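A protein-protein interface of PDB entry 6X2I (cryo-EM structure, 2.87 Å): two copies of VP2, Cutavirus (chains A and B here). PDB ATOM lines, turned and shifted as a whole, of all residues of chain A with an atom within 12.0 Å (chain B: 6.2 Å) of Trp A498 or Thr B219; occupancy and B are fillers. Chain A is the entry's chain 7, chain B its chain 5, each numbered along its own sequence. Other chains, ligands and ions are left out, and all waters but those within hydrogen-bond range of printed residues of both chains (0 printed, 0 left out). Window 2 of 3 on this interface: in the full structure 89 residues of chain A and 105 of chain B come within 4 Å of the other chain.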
ATOM      1  N   ARG A 493      11.617  17.175  -1.073  1.00  0.00           N
ATOM      2  CA  ARG A 493      10.956  17.710   0.106  1.00  0.00           C
ATOM      3  C   ARG A 493      11.800  17.445   1.344  1.00  0.00           C
ATOM      4  O   ARG A 493      12.379  16.368   1.494  1.00  0.00           O
ATOM      5  CB  ARG A 493       9.579  17.088   0.292  1.00  0.00           C
ATOM      6  CG  ARG A 493       8.802  17.718   1.402  1.00  0.00           C
ATOM      7  CD  ARG A 493       7.507  17.023   1.631  1.00  0.00           C
ATOM      8  NE  ARG A 493       7.725  15.689   2.163  1.00  0.00           N
ATOM      9  CZ  ARG A 493       7.938  15.432   3.447  1.00  0.00           C
ATOM     10  NH1 ARG A 493       7.962  16.418   4.322  1.00  0.00           N
ATOM     11  NH2 ARG A 493       8.131  14.190   3.853  1.00  0.00           N
ATOM     12  N   THR A 494      11.860  18.425   2.230  1.00  0.00           N
ATOM     13  CA  THR A 494      12.594  18.350   3.479  1.00  0.00           C
ATOM     14  C   THR A 494      11.688  18.828   4.614  1.00  0.00           C
ATOM     15  O   THR A 494      10.733  19.560   4.370  1.00  0.00           O
ATOM     16  CB  THR A 494      13.863  19.211   3.426  1.00  0.00           C
ATOM     17  OG1 THR A 494      13.512  20.565   3.129  1.00  0.00           O
ATOM     18  CG2 THR A 494      14.802  18.696   2.351  1.00  0.00           C
ATOM     19  N   PRO A 495      11.963  18.404   5.842  1.00  0.00           N
ATOM     20  CA  PRO A 495      11.091  18.807   6.958  1.00  0.00           C
ATOM     21  C   PRO A 495      11.119  20.309   7.186  1.00  0.00           C
ATOM     22  O   PRO A 495      12.183  20.916   7.293  1.00  0.00           O
ATOM     23  CB  PRO A 495      11.686  18.049   8.148  1.00  0.00           C
ATOM     24  CG  PRO A 495      12.372  16.904   7.550  1.00  0.00           C
ATOM     25  CD  PRO A 495      12.946  17.409   6.270  1.00  0.00           C
ATOM     26  N   ARG A 496       9.934  20.910   7.240  1.00  0.00           N
ATOM     27  CA  ARG A 496       9.788  22.294   7.660  1.00  0.00           C
ATOM     28  C   ARG A 496       9.316  22.453   9.094  1.00  0.00           C
ATOM     29  O   ARG A 496       9.076  23.579   9.514  1.00  0.00           O
ATOM     30  CB  ARG A 496       8.835  23.053   6.739  1.00  0.00           C
ATOM     31  CG  ARG A 496       9.381  23.276   5.352  1.00  0.00           C
ATOM     32  CD  ARG A 496       8.420  24.069   4.499  1.00  0.00           C
ATOM     33  NE  ARG A 496       8.240  25.432   4.988  1.00  0.00           N
ATOM     34  CZ  ARG A 496       7.379  26.300   4.471  1.00  0.00           C
ATOM     35  NH1 ARG A 496       7.277  27.519   4.970  1.00  0.00           N
ATOM     36  NH2 ARG A 496       6.614  25.945   3.451  1.00  0.00           N
ATOM     37  N   GLN A 497       9.150  21.376   9.848  1.00  0.00           N
ATOM     38  CA  GLN A 497       8.545  21.475  11.162  1.00  0.00           C
ATOM     39  C   GLN A 497       9.343  20.667  12.171  1.00  0.00           C
ATOM     40  O   GLN A 497      10.216  19.875  11.817  1.00  0.00           O
ATOM     41  CB  GLN A 497       7.097  20.995  11.127  1.00  0.00           C
ATOM     42  CG  GLN A 497       6.963  19.531  10.849  1.00  0.00           C
ATOM     43  CD  GLN A 497       5.538  19.116  10.684  1.00  0.00           C
ATOM     44  OE1 GLN A 497       4.699  19.919  10.319  1.00  0.00           O
ATOM     45  NE2 GLN A 497       5.246  17.866  10.976  1.00  0.00           N
ATOM     46  N   TRP A 498       9.052  20.905  13.451  1.00  0.00           N
ATOM     47  CA  TRP A 498       9.674  20.152  14.536  1.00  0.00           C
ATOM     48  C   TRP A 498       9.059  18.770  14.694  1.00  0.00           C
ATOM     49  O   TRP A 498       9.771  17.763  14.716  1.00  0.00           O
ATOM     50  CB  TRP A 498       9.540  20.931  15.840  1.00  0.00           C
ATOM     51  CG  TRP A 498       9.993  20.191  17.049  1.00  0.00           C
ATOM     52  CD1 TRP A 498       9.209  19.526  17.932  1.00  0.00           C
ATOM     53  CD2 TRP A 498      11.327  20.081  17.537  1.00  0.00           C
ATOM     54  NE1 TRP A 498       9.971  18.979  18.923  1.00  0.00           N
ATOM     55  CE2 TRP A 498      11.278  19.312  18.706  1.00  0.00           C
ATOM     56  CE3 TRP A 498      12.560  20.550  17.092  1.00  0.00           C
ATOM     57  CZ2 TRP A 498      12.411  19.001  19.436  1.00  0.00           C
ATOM     58  CZ3 TRP A 498      13.681  20.235  17.816  1.00  0.00           C
ATOM     59  CH2 TRP A 498      13.601  19.469  18.975  1.00  0.00           C
ATOM     60  N   ASN A 499       7.742  18.703  14.807  1.00  0.00           N
ATOM     61  CA  ASN A 499       7.053  17.455  15.069  1.00  0.00           C
ATOM     62  C   ASN A 499       7.004  16.578  13.826  1.00  0.00           C
ATOM     63  O   ASN A 499       7.225  17.028  12.702  1.00  0.00           O
ATOM     64  CB  ASN A 499       5.649  17.724  15.589  1.00  0.00           C
ATOM     65  CG  ASN A 499       4.856  18.597  14.667  1.00  0.00           C
ATOM     66  OD1 ASN A 499       5.412  19.272  13.817  1.00  0.00           O
ATOM     67  ND2 ASN A 499       3.548  18.583  14.820  1.00  0.00           N
ATOM     68  N   THR A 500       6.730  15.300  14.047  1.00  0.00           N
ATOM     69  CA  THR A 500       6.662  14.349  12.956  1.00  0.00           C
ATOM     70  C   THR A 500       5.447  14.619  12.076  1.00  0.00           C
ATOM     71  O   THR A 500       4.461  15.216  12.503  1.00  0.00           O
ATOM     72  CB  THR A 500       6.609  12.927  13.508  1.00  0.00           C
ATOM     73  OG1 THR A 500       5.472  12.792  14.361  1.00  0.00           O
ATOM     74  CG2 THR A 500       7.834  12.638  14.307  1.00  0.00           C
ATOM     75  N   TYR A 501       5.529  14.172  10.827  1.00  0.00           N
ATOM     76  CA  TYR A 501       4.410  14.250   9.907  1.00  0.00           C
ATOM     77  C   TYR A 501       3.509  13.029  10.046  1.00  0.00           C
ATOM     78  O   TYR A 501       3.814  12.076  10.761  1.00  0.00           O
ATOM     79  CB  TYR A 501       4.903  14.338   8.465  1.00  0.00           C
ATOM     80  CG  TYR A 501       5.600  15.614   8.089  1.00  0.00           C
ATOM     81  CD1 TYR A 501       4.896  16.676   7.559  1.00  0.00           C
ATOM     82  CD2 TYR A 501       6.961  15.753   8.252  1.00  0.00           C
ATOM     83  CE1 TYR A 501       5.528  17.836   7.210  1.00  0.00           C
ATOM     84  CE2 TYR A 501       7.600  16.910   7.909  1.00  0.00           C
ATOM     85  CZ  TYR A 501       6.883  17.949   7.388  1.00  0.00           C
ATOM     86  OH  TYR A 501       7.526  19.109   7.044  1.00  0.00           O
ATOM     87  N   ASN A 502       2.396  13.056   9.322  1.00  0.00           N
ATOM     88  CA  ASN A 502       1.621  11.860   9.023  1.00  0.00           C
ATOM     89  C   ASN A 502       1.960  11.474   7.597  1.00  0.00           C
ATOM     90  O   ASN A 502       1.500  12.112   6.649  1.00  0.00           O
ATOM     91  CB  ASN A 502       0.124  12.101   9.169  1.00  0.00           C
ATOM     92  CG  ASN A 502      -0.329  12.080  10.590  1.00  0.00           C
ATOM     93  OD1 ASN A 502      -0.525  11.018  11.166  1.00  0.00           O
ATOM     94  ND2 ASN A 502      -0.487  13.253  11.179  1.00  0.00           N
ATOM     95  N   LEU A 503       2.719  10.443   7.448  1.00  0.00           N
ATOM     96  CA  LEU A 503       3.174  10.168   6.106  1.00  0.00           C
ATOM     97  C   LEU A 503       2.076   9.455   5.329  1.00  0.00           C
ATOM     98  O   LEU A 503       1.222   8.797   5.924  1.00  0.00           O
ATOM     99  CB  LEU A 503       4.440   9.333   6.151  1.00  0.00           C
ATOM    100  CG  LEU A 503       5.590  10.053   6.849  1.00  0.00           C
ATOM    101  CD1 LEU A 503       6.789   9.150   6.971  1.00  0.00           C
ATOM    102  CD2 LEU A 503       5.955  11.327   6.126  1.00  0.00           C
ATOM    103  N   PRO A 534       0.639  18.483   4.470  1.00  0.00           N
ATOM    104  CA  PRO A 534       0.327  19.908   4.545  1.00  0.00           C
ATOM    105  C   PRO A 534       1.538  20.784   4.277  1.00  0.00           C
ATOM    106  O   PRO A 534       2.688  20.360   4.365  1.00  0.00           O
ATOM    107  CB  PRO A 534      -0.157  20.078   5.984  1.00  0.00           C
ATOM    108  CG  PRO A 534       0.544  19.032   6.714  1.00  0.00           C
ATOM    109  CD  PRO A 534       0.632  17.861   5.800  1.00  0.00           C
ATOM    110  N   ASN A 535       1.247  22.038   3.943  1.00  0.00           N
ATOM    111  CA  ASN A 535       2.276  23.057   3.814  1.00  0.00           C
ATOM    112  C   ASN A 535       1.612  24.414   3.967  1.00  0.00           C
ATOM    113  O   ASN A 535       0.392  24.537   3.863  1.00  0.00           O
ATOM    114  CB  ASN A 535       3.010  22.941   2.479  1.00  0.00           C
ATOM    115  CG  ASN A 535       4.270  23.764   2.435  1.00  0.00           C
ATOM    116  OD1 ASN A 535       4.870  24.058   3.463  1.00  0.00           O
ATOM    117  ND2 ASN A 535       4.696  24.118   1.236  1.00  0.00           N
ATOM    118  N   TYR A 536       2.423  25.430   4.236  1.00  0.00           N
ATOM    119  CA  TYR A 536       1.891  26.770   4.415  1.00  0.00           C
ATOM    120  C   TYR A 536       1.671  27.436   3.067  1.00  0.00           C
ATOM    121  O   TYR A 536       2.585  27.499   2.242  1.00  0.00           O
ATOM    122  CB  TYR A 536       2.840  27.631   5.243  1.00  0.00           C
ATOM    123  CG  TYR A 536       3.120  27.137   6.632  1.00  0.00           C
ATOM    124  CD1 TYR A 536       2.225  27.361   7.660  1.00  0.00           C
ATOM    125  CD2 TYR A 536       4.314  26.507   6.931  1.00  0.00           C
ATOM    126  CE1 TYR A 536       2.490  26.929   8.932  1.00  0.00           C
ATOM    127  CE2 TYR A 536       4.587  26.077   8.197  1.00  0.00           C
ATOM    128  CZ  TYR A 536       3.675  26.290   9.195  1.00  0.00           C
ATOM    129  OH  TYR A 536       3.953  25.857  10.466  1.00  0.00           O
ATOM    130  N   PHE B 214       4.268  22.751  13.658  1.00  0.00           N
ATOM    131  CA  PHE B 214       4.956  23.602  14.623  1.00  0.00           C
ATOM    132  C   PHE B 214       6.405  23.766  14.198  1.00  0.00           C
ATOM    133  O   PHE B 214       7.161  22.791  14.181  1.00  0.00           O
ATOM    134  CB  PHE B 214       4.858  23.020  16.029  1.00  0.00           C
ATOM    135  CG  PHE B 214       5.847  23.590  16.982  1.00  0.00           C
ATOM    136  CD1 PHE B 214       5.733  24.882  17.427  1.00  0.00           C
ATOM    137  CD2 PHE B 214       6.881  22.820  17.454  1.00  0.00           C
ATOM    138  CE1 PHE B 214       6.645  25.402  18.295  1.00  0.00           C
ATOM    139  CE2 PHE B 214       7.789  23.338  18.332  1.00  0.00           C
ATOM    140  CZ  PHE B 214       7.670  24.633  18.752  1.00  0.00           C
ATOM    141  N   THR B 215       6.789  24.987  13.847  1.00  0.00           N
ATOM    142  CA  THR B 215       8.144  25.271  13.379  1.00  0.00           C
ATOM    143  C   THR B 215       8.821  26.261  14.314  1.00  0.00           C
ATOM    144  O   THR B 215       8.392  27.427  14.385  1.00  0.00           O
ATOM    145  CB  THR B 215       8.118  25.848  11.967  1.00  0.00           C
ATOM    146  OG1 THR B 215       7.712  27.213  12.034  1.00  0.00           O
ATOM    147  CG2 THR B 215       7.083  25.135  11.144  1.00  0.00           C
ATOM    148  N   PRO B 216       9.855  25.875  15.052  1.00  0.00           N
ATOM    149  CA  PRO B 216      10.693  26.867  15.726  1.00  0.00           C
ATOM    150  C   PRO B 216      11.669  27.523  14.761  1.00  0.00           C
ATOM    151  O   PRO B 216      11.989  26.993  13.700  1.00  0.00           O
ATOM    152  CB  PRO B 216      11.445  26.033  16.763  1.00  0.00           C
ATOM    153  CG  PRO B 216      10.611  24.849  16.956  1.00  0.00           C
ATOM    154  CD  PRO B 216      10.067  24.536  15.611  1.00  0.00           C
ATOM    155  N   LEU B 217      12.149  28.701  15.152  1.00  0.00           N
ATOM    156  CA  LEU B 217      13.180  29.346  14.350  1.00  0.00           C
ATOM    157  C   LEU B 217      14.519  28.657  14.507  1.00  0.00           C
ATOM    158  O   LEU B 217      15.330  28.667  13.577  1.00  0.00           O
ATOM    159  CB  LEU B 217      13.334  30.823  14.708  1.00  0.00           C
ATOM    160  CG  LEU B 217      12.306  31.880  14.321  1.00  0.00           C
ATOM    161  CD1 LEU B 217      10.927  31.603  14.861  1.00  0.00           C
ATOM    162  CD2 LEU B 217      12.789  33.203  14.813  1.00  0.00           C
ATOM    163  N   GLU B 218      14.776  28.071  15.676  1.00  0.00           N
ATOM    164  CA  GLU B 218      16.078  27.476  15.942  1.00  0.00           C
ATOM    165  C   GLU B 218      16.411  26.388  14.940  1.00  0.00           C
ATOM    166  O   GLU B 218      17.552  26.286  14.485  1.00  0.00           O
ATOM    167  CB  GLU B 218      16.110  26.931  17.365  1.00  0.00           C
ATOM    168  CG  GLU B 218      16.171  28.005  18.422  1.00  0.00           C
ATOM    169  CD  GLU B 218      14.844  28.682  18.662  1.00  0.00           C
ATOM    170  OE1 GLU B 218      13.879  28.395  17.933  1.00  0.00           O
ATOM    171  OE2 GLU B 218      14.765  29.507  19.591  1.00  0.00           O
ATOM    172  N   THR B 219      15.428  25.576  14.575  1.00  0.00           N
ATOM    173  CA  THR B 219      15.675  24.474  13.659  1.00  0.00           C
ATOM    174  C   THR B 219      15.707  24.925  12.205  1.00  0.00           C
ATOM    175  O   THR B 219      16.361  24.288  11.380  1.00  0.00           O
ATOM    176  CB  THR B 219      14.610  23.403  13.864  1.00  0.00           C
ATOM    177  OG1 THR B 219      14.608  23.009  15.239  1.00  0.00           O
ATOM    178  CG2 THR B 219      14.915  22.184  13.029  1.00  0.00           C
ATOM    179  N   MET B 220      15.003  25.998  11.862  1.00  0.00           N
ATOM    180  CA  MET B 220      14.887  26.368  10.457  1.00  0.00           C
ATOM    181  C   MET B 220      16.063  27.186   9.945  1.00  0.00           C
ATOM    182  O   MET B 220      16.554  26.934   8.842  1.00  0.00           O
ATOM    183  CB  MET B 220      13.580  27.114  10.225  1.00  0.00           C
ATOM    184  CG  MET B 220      12.356  26.226  10.306  1.00  0.00           C
ATOM    185  SD  MET B 220      12.321  25.009   8.976  1.00  0.00           S
ATOM    186  CE  MET B 220      12.817  23.519   9.830  1.00  0.00           C
ATOM    187  N   ILE B 221      16.528  28.175  10.703  1.00  0.00           N
ATOM    188  CA  ILE B 221      17.451  29.163  10.162  1.00  0.00           C
ATOM    189  C   ILE B 221      18.600  29.408  11.126  1.00  0.00           C
ATOM    190  O   ILE B 221      18.498  29.171  12.327  1.00  0.00           O
ATOM    191  CB  ILE B 221      16.731  30.485   9.832  1.00  0.00           C
ATOM    192  CG1 ILE B 221      15.994  31.008  11.056  1.00  0.00           C
ATOM    193  CG2 ILE B 221      15.770  30.301   8.675  1.00  0.00           C
ATOM    194  CD1 ILE B 221      15.328  32.314  10.825  1.00  0.00           C
ATOM    195  N   ILE B 223      21.115  31.466  13.412  1.00  0.00           N
ATOM    196  CA  ILE B 223      20.901  32.566  14.337  1.00  0.00           C
ATOM    197  C   ILE B 223      22.257  33.147  14.692  1.00  0.00           C
ATOM    198  O   ILE B 223      23.199  32.403  14.970  1.00  0.00           O
ATOM    199  CB  ILE B 223      20.152  32.093  15.594  1.00  0.00           C
ATOM    200  CG1 ILE B 223      18.769  31.583  15.200  1.00  0.00           C
ATOM    201  CG2 ILE B 223      20.049  33.206  16.605  1.00  0.00           C
ATOM    202  CD1 ILE B 223      18.059  30.842  16.286  1.00  0.00           C
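Of the printed residues of chain B, Pro A495 touches Met B220 (3.7 Å).
Printed residues of chain B within 4 Å of Arg A496: Thr B215 (3.0 Å) and Met B220 (3.6 Å).
Printed residues of chain B within 4 Å of Gln A497: Phe B214 (3.5 Å) and Thr B215 (3.9 Å).
Trp A498 touches just these residues of chain B: Phe B214 (2.8 Å), Pro B216 (3.7 Å) and Thr B219 (3.7 Å).
Asn A502 touches none of the printed residues of chain B.
Of the printed residues of chain B, Tyr A536 touches Thr B215.
Of chain A, only Gln A497, Trp A498 and Asn A499 come within 4 Å of Phe B214.
Thr B215 touches just these residues of chain A: Arg A496 (3.0 Å), Gln A497 (3.9 Å) and Tyr A536 (3.3 Å).
Of chain A, only Trp A498 (3.7 Å) comes within 4 Å of Pro B216.
Of chain A, only Trp A498 comes within 4 Å of Thr B219.
Met B220 touches just these residues of chain A: Pro A495 (3.7 Å) and Arg A496 (3.6 Å).
Ile B221 touches none of the printed residues of chain A.
The nearest residue of chain B that does not touch Trp A498 is Thr B215 (4.5 Å).
N of Arg A496 lies within hydrogen-bond range of OH of Tyr A501 (3.0 Å).
The backbone carbonyl oxygen of Asn A499 is in hydrogen-bond range of the side-chain amide nitrogen of Gln A497, at 2.8 Å.
OD1 of Asn A535 is in hydrogen-bond range of NH2 of Arg A496.
NE2 of Gln A497 sits at hydrogen-bond distance from O of Thr A500 (3.2 Å).
Hydrophobic or aromatic side chains of chain B within 4 Å of the printed part of chain A: Phe B214, Pro B216 and Met B220.
Hydrophobic or aromatic side chains of chain A within 4 Å of the printed part of chain B: Trp A498 and Tyr A536.
Among the printed residues, no Asp or Glu carboxylate lies within 4 Å of a Lys or Arg side-chain nitrogen of the other chain.
The backbone carbonyl oxygen (O) of Phe B214 is in hydrogen-bond range of the backbone NH (N) of Trp A498 (2.8 Å).
The backbone carbonyl oxygen of Arg A496 lies close to the side-chain sulfur of Met B220 (3.6 Å).
Pro A495 touches Met B220 (O to CE, 3.7 Å).
O of Arg A496 touches CG2 of Thr B215, at 3.0 Å.
O of Phe B214 touches CB of Gln A497, at 3.5 Å.
CG2 of Thr B215 touches CA of Gln A497 (3.9 Å).
CB of Trp A498 touches CD of Pro B216, 3.7 Å away.
Thr B219 touches Trp A498.
OD1 of Asn A499 touches N of Phe B214, 3.7 Å away.
OH of Tyr A536 touches CG2 of Thr B215, at 3.3 Å.
No position is printed for both chains.
Of the 10 pairs that touch across the chains among the printed residues, none has its exchanged pair printed and touching as well.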
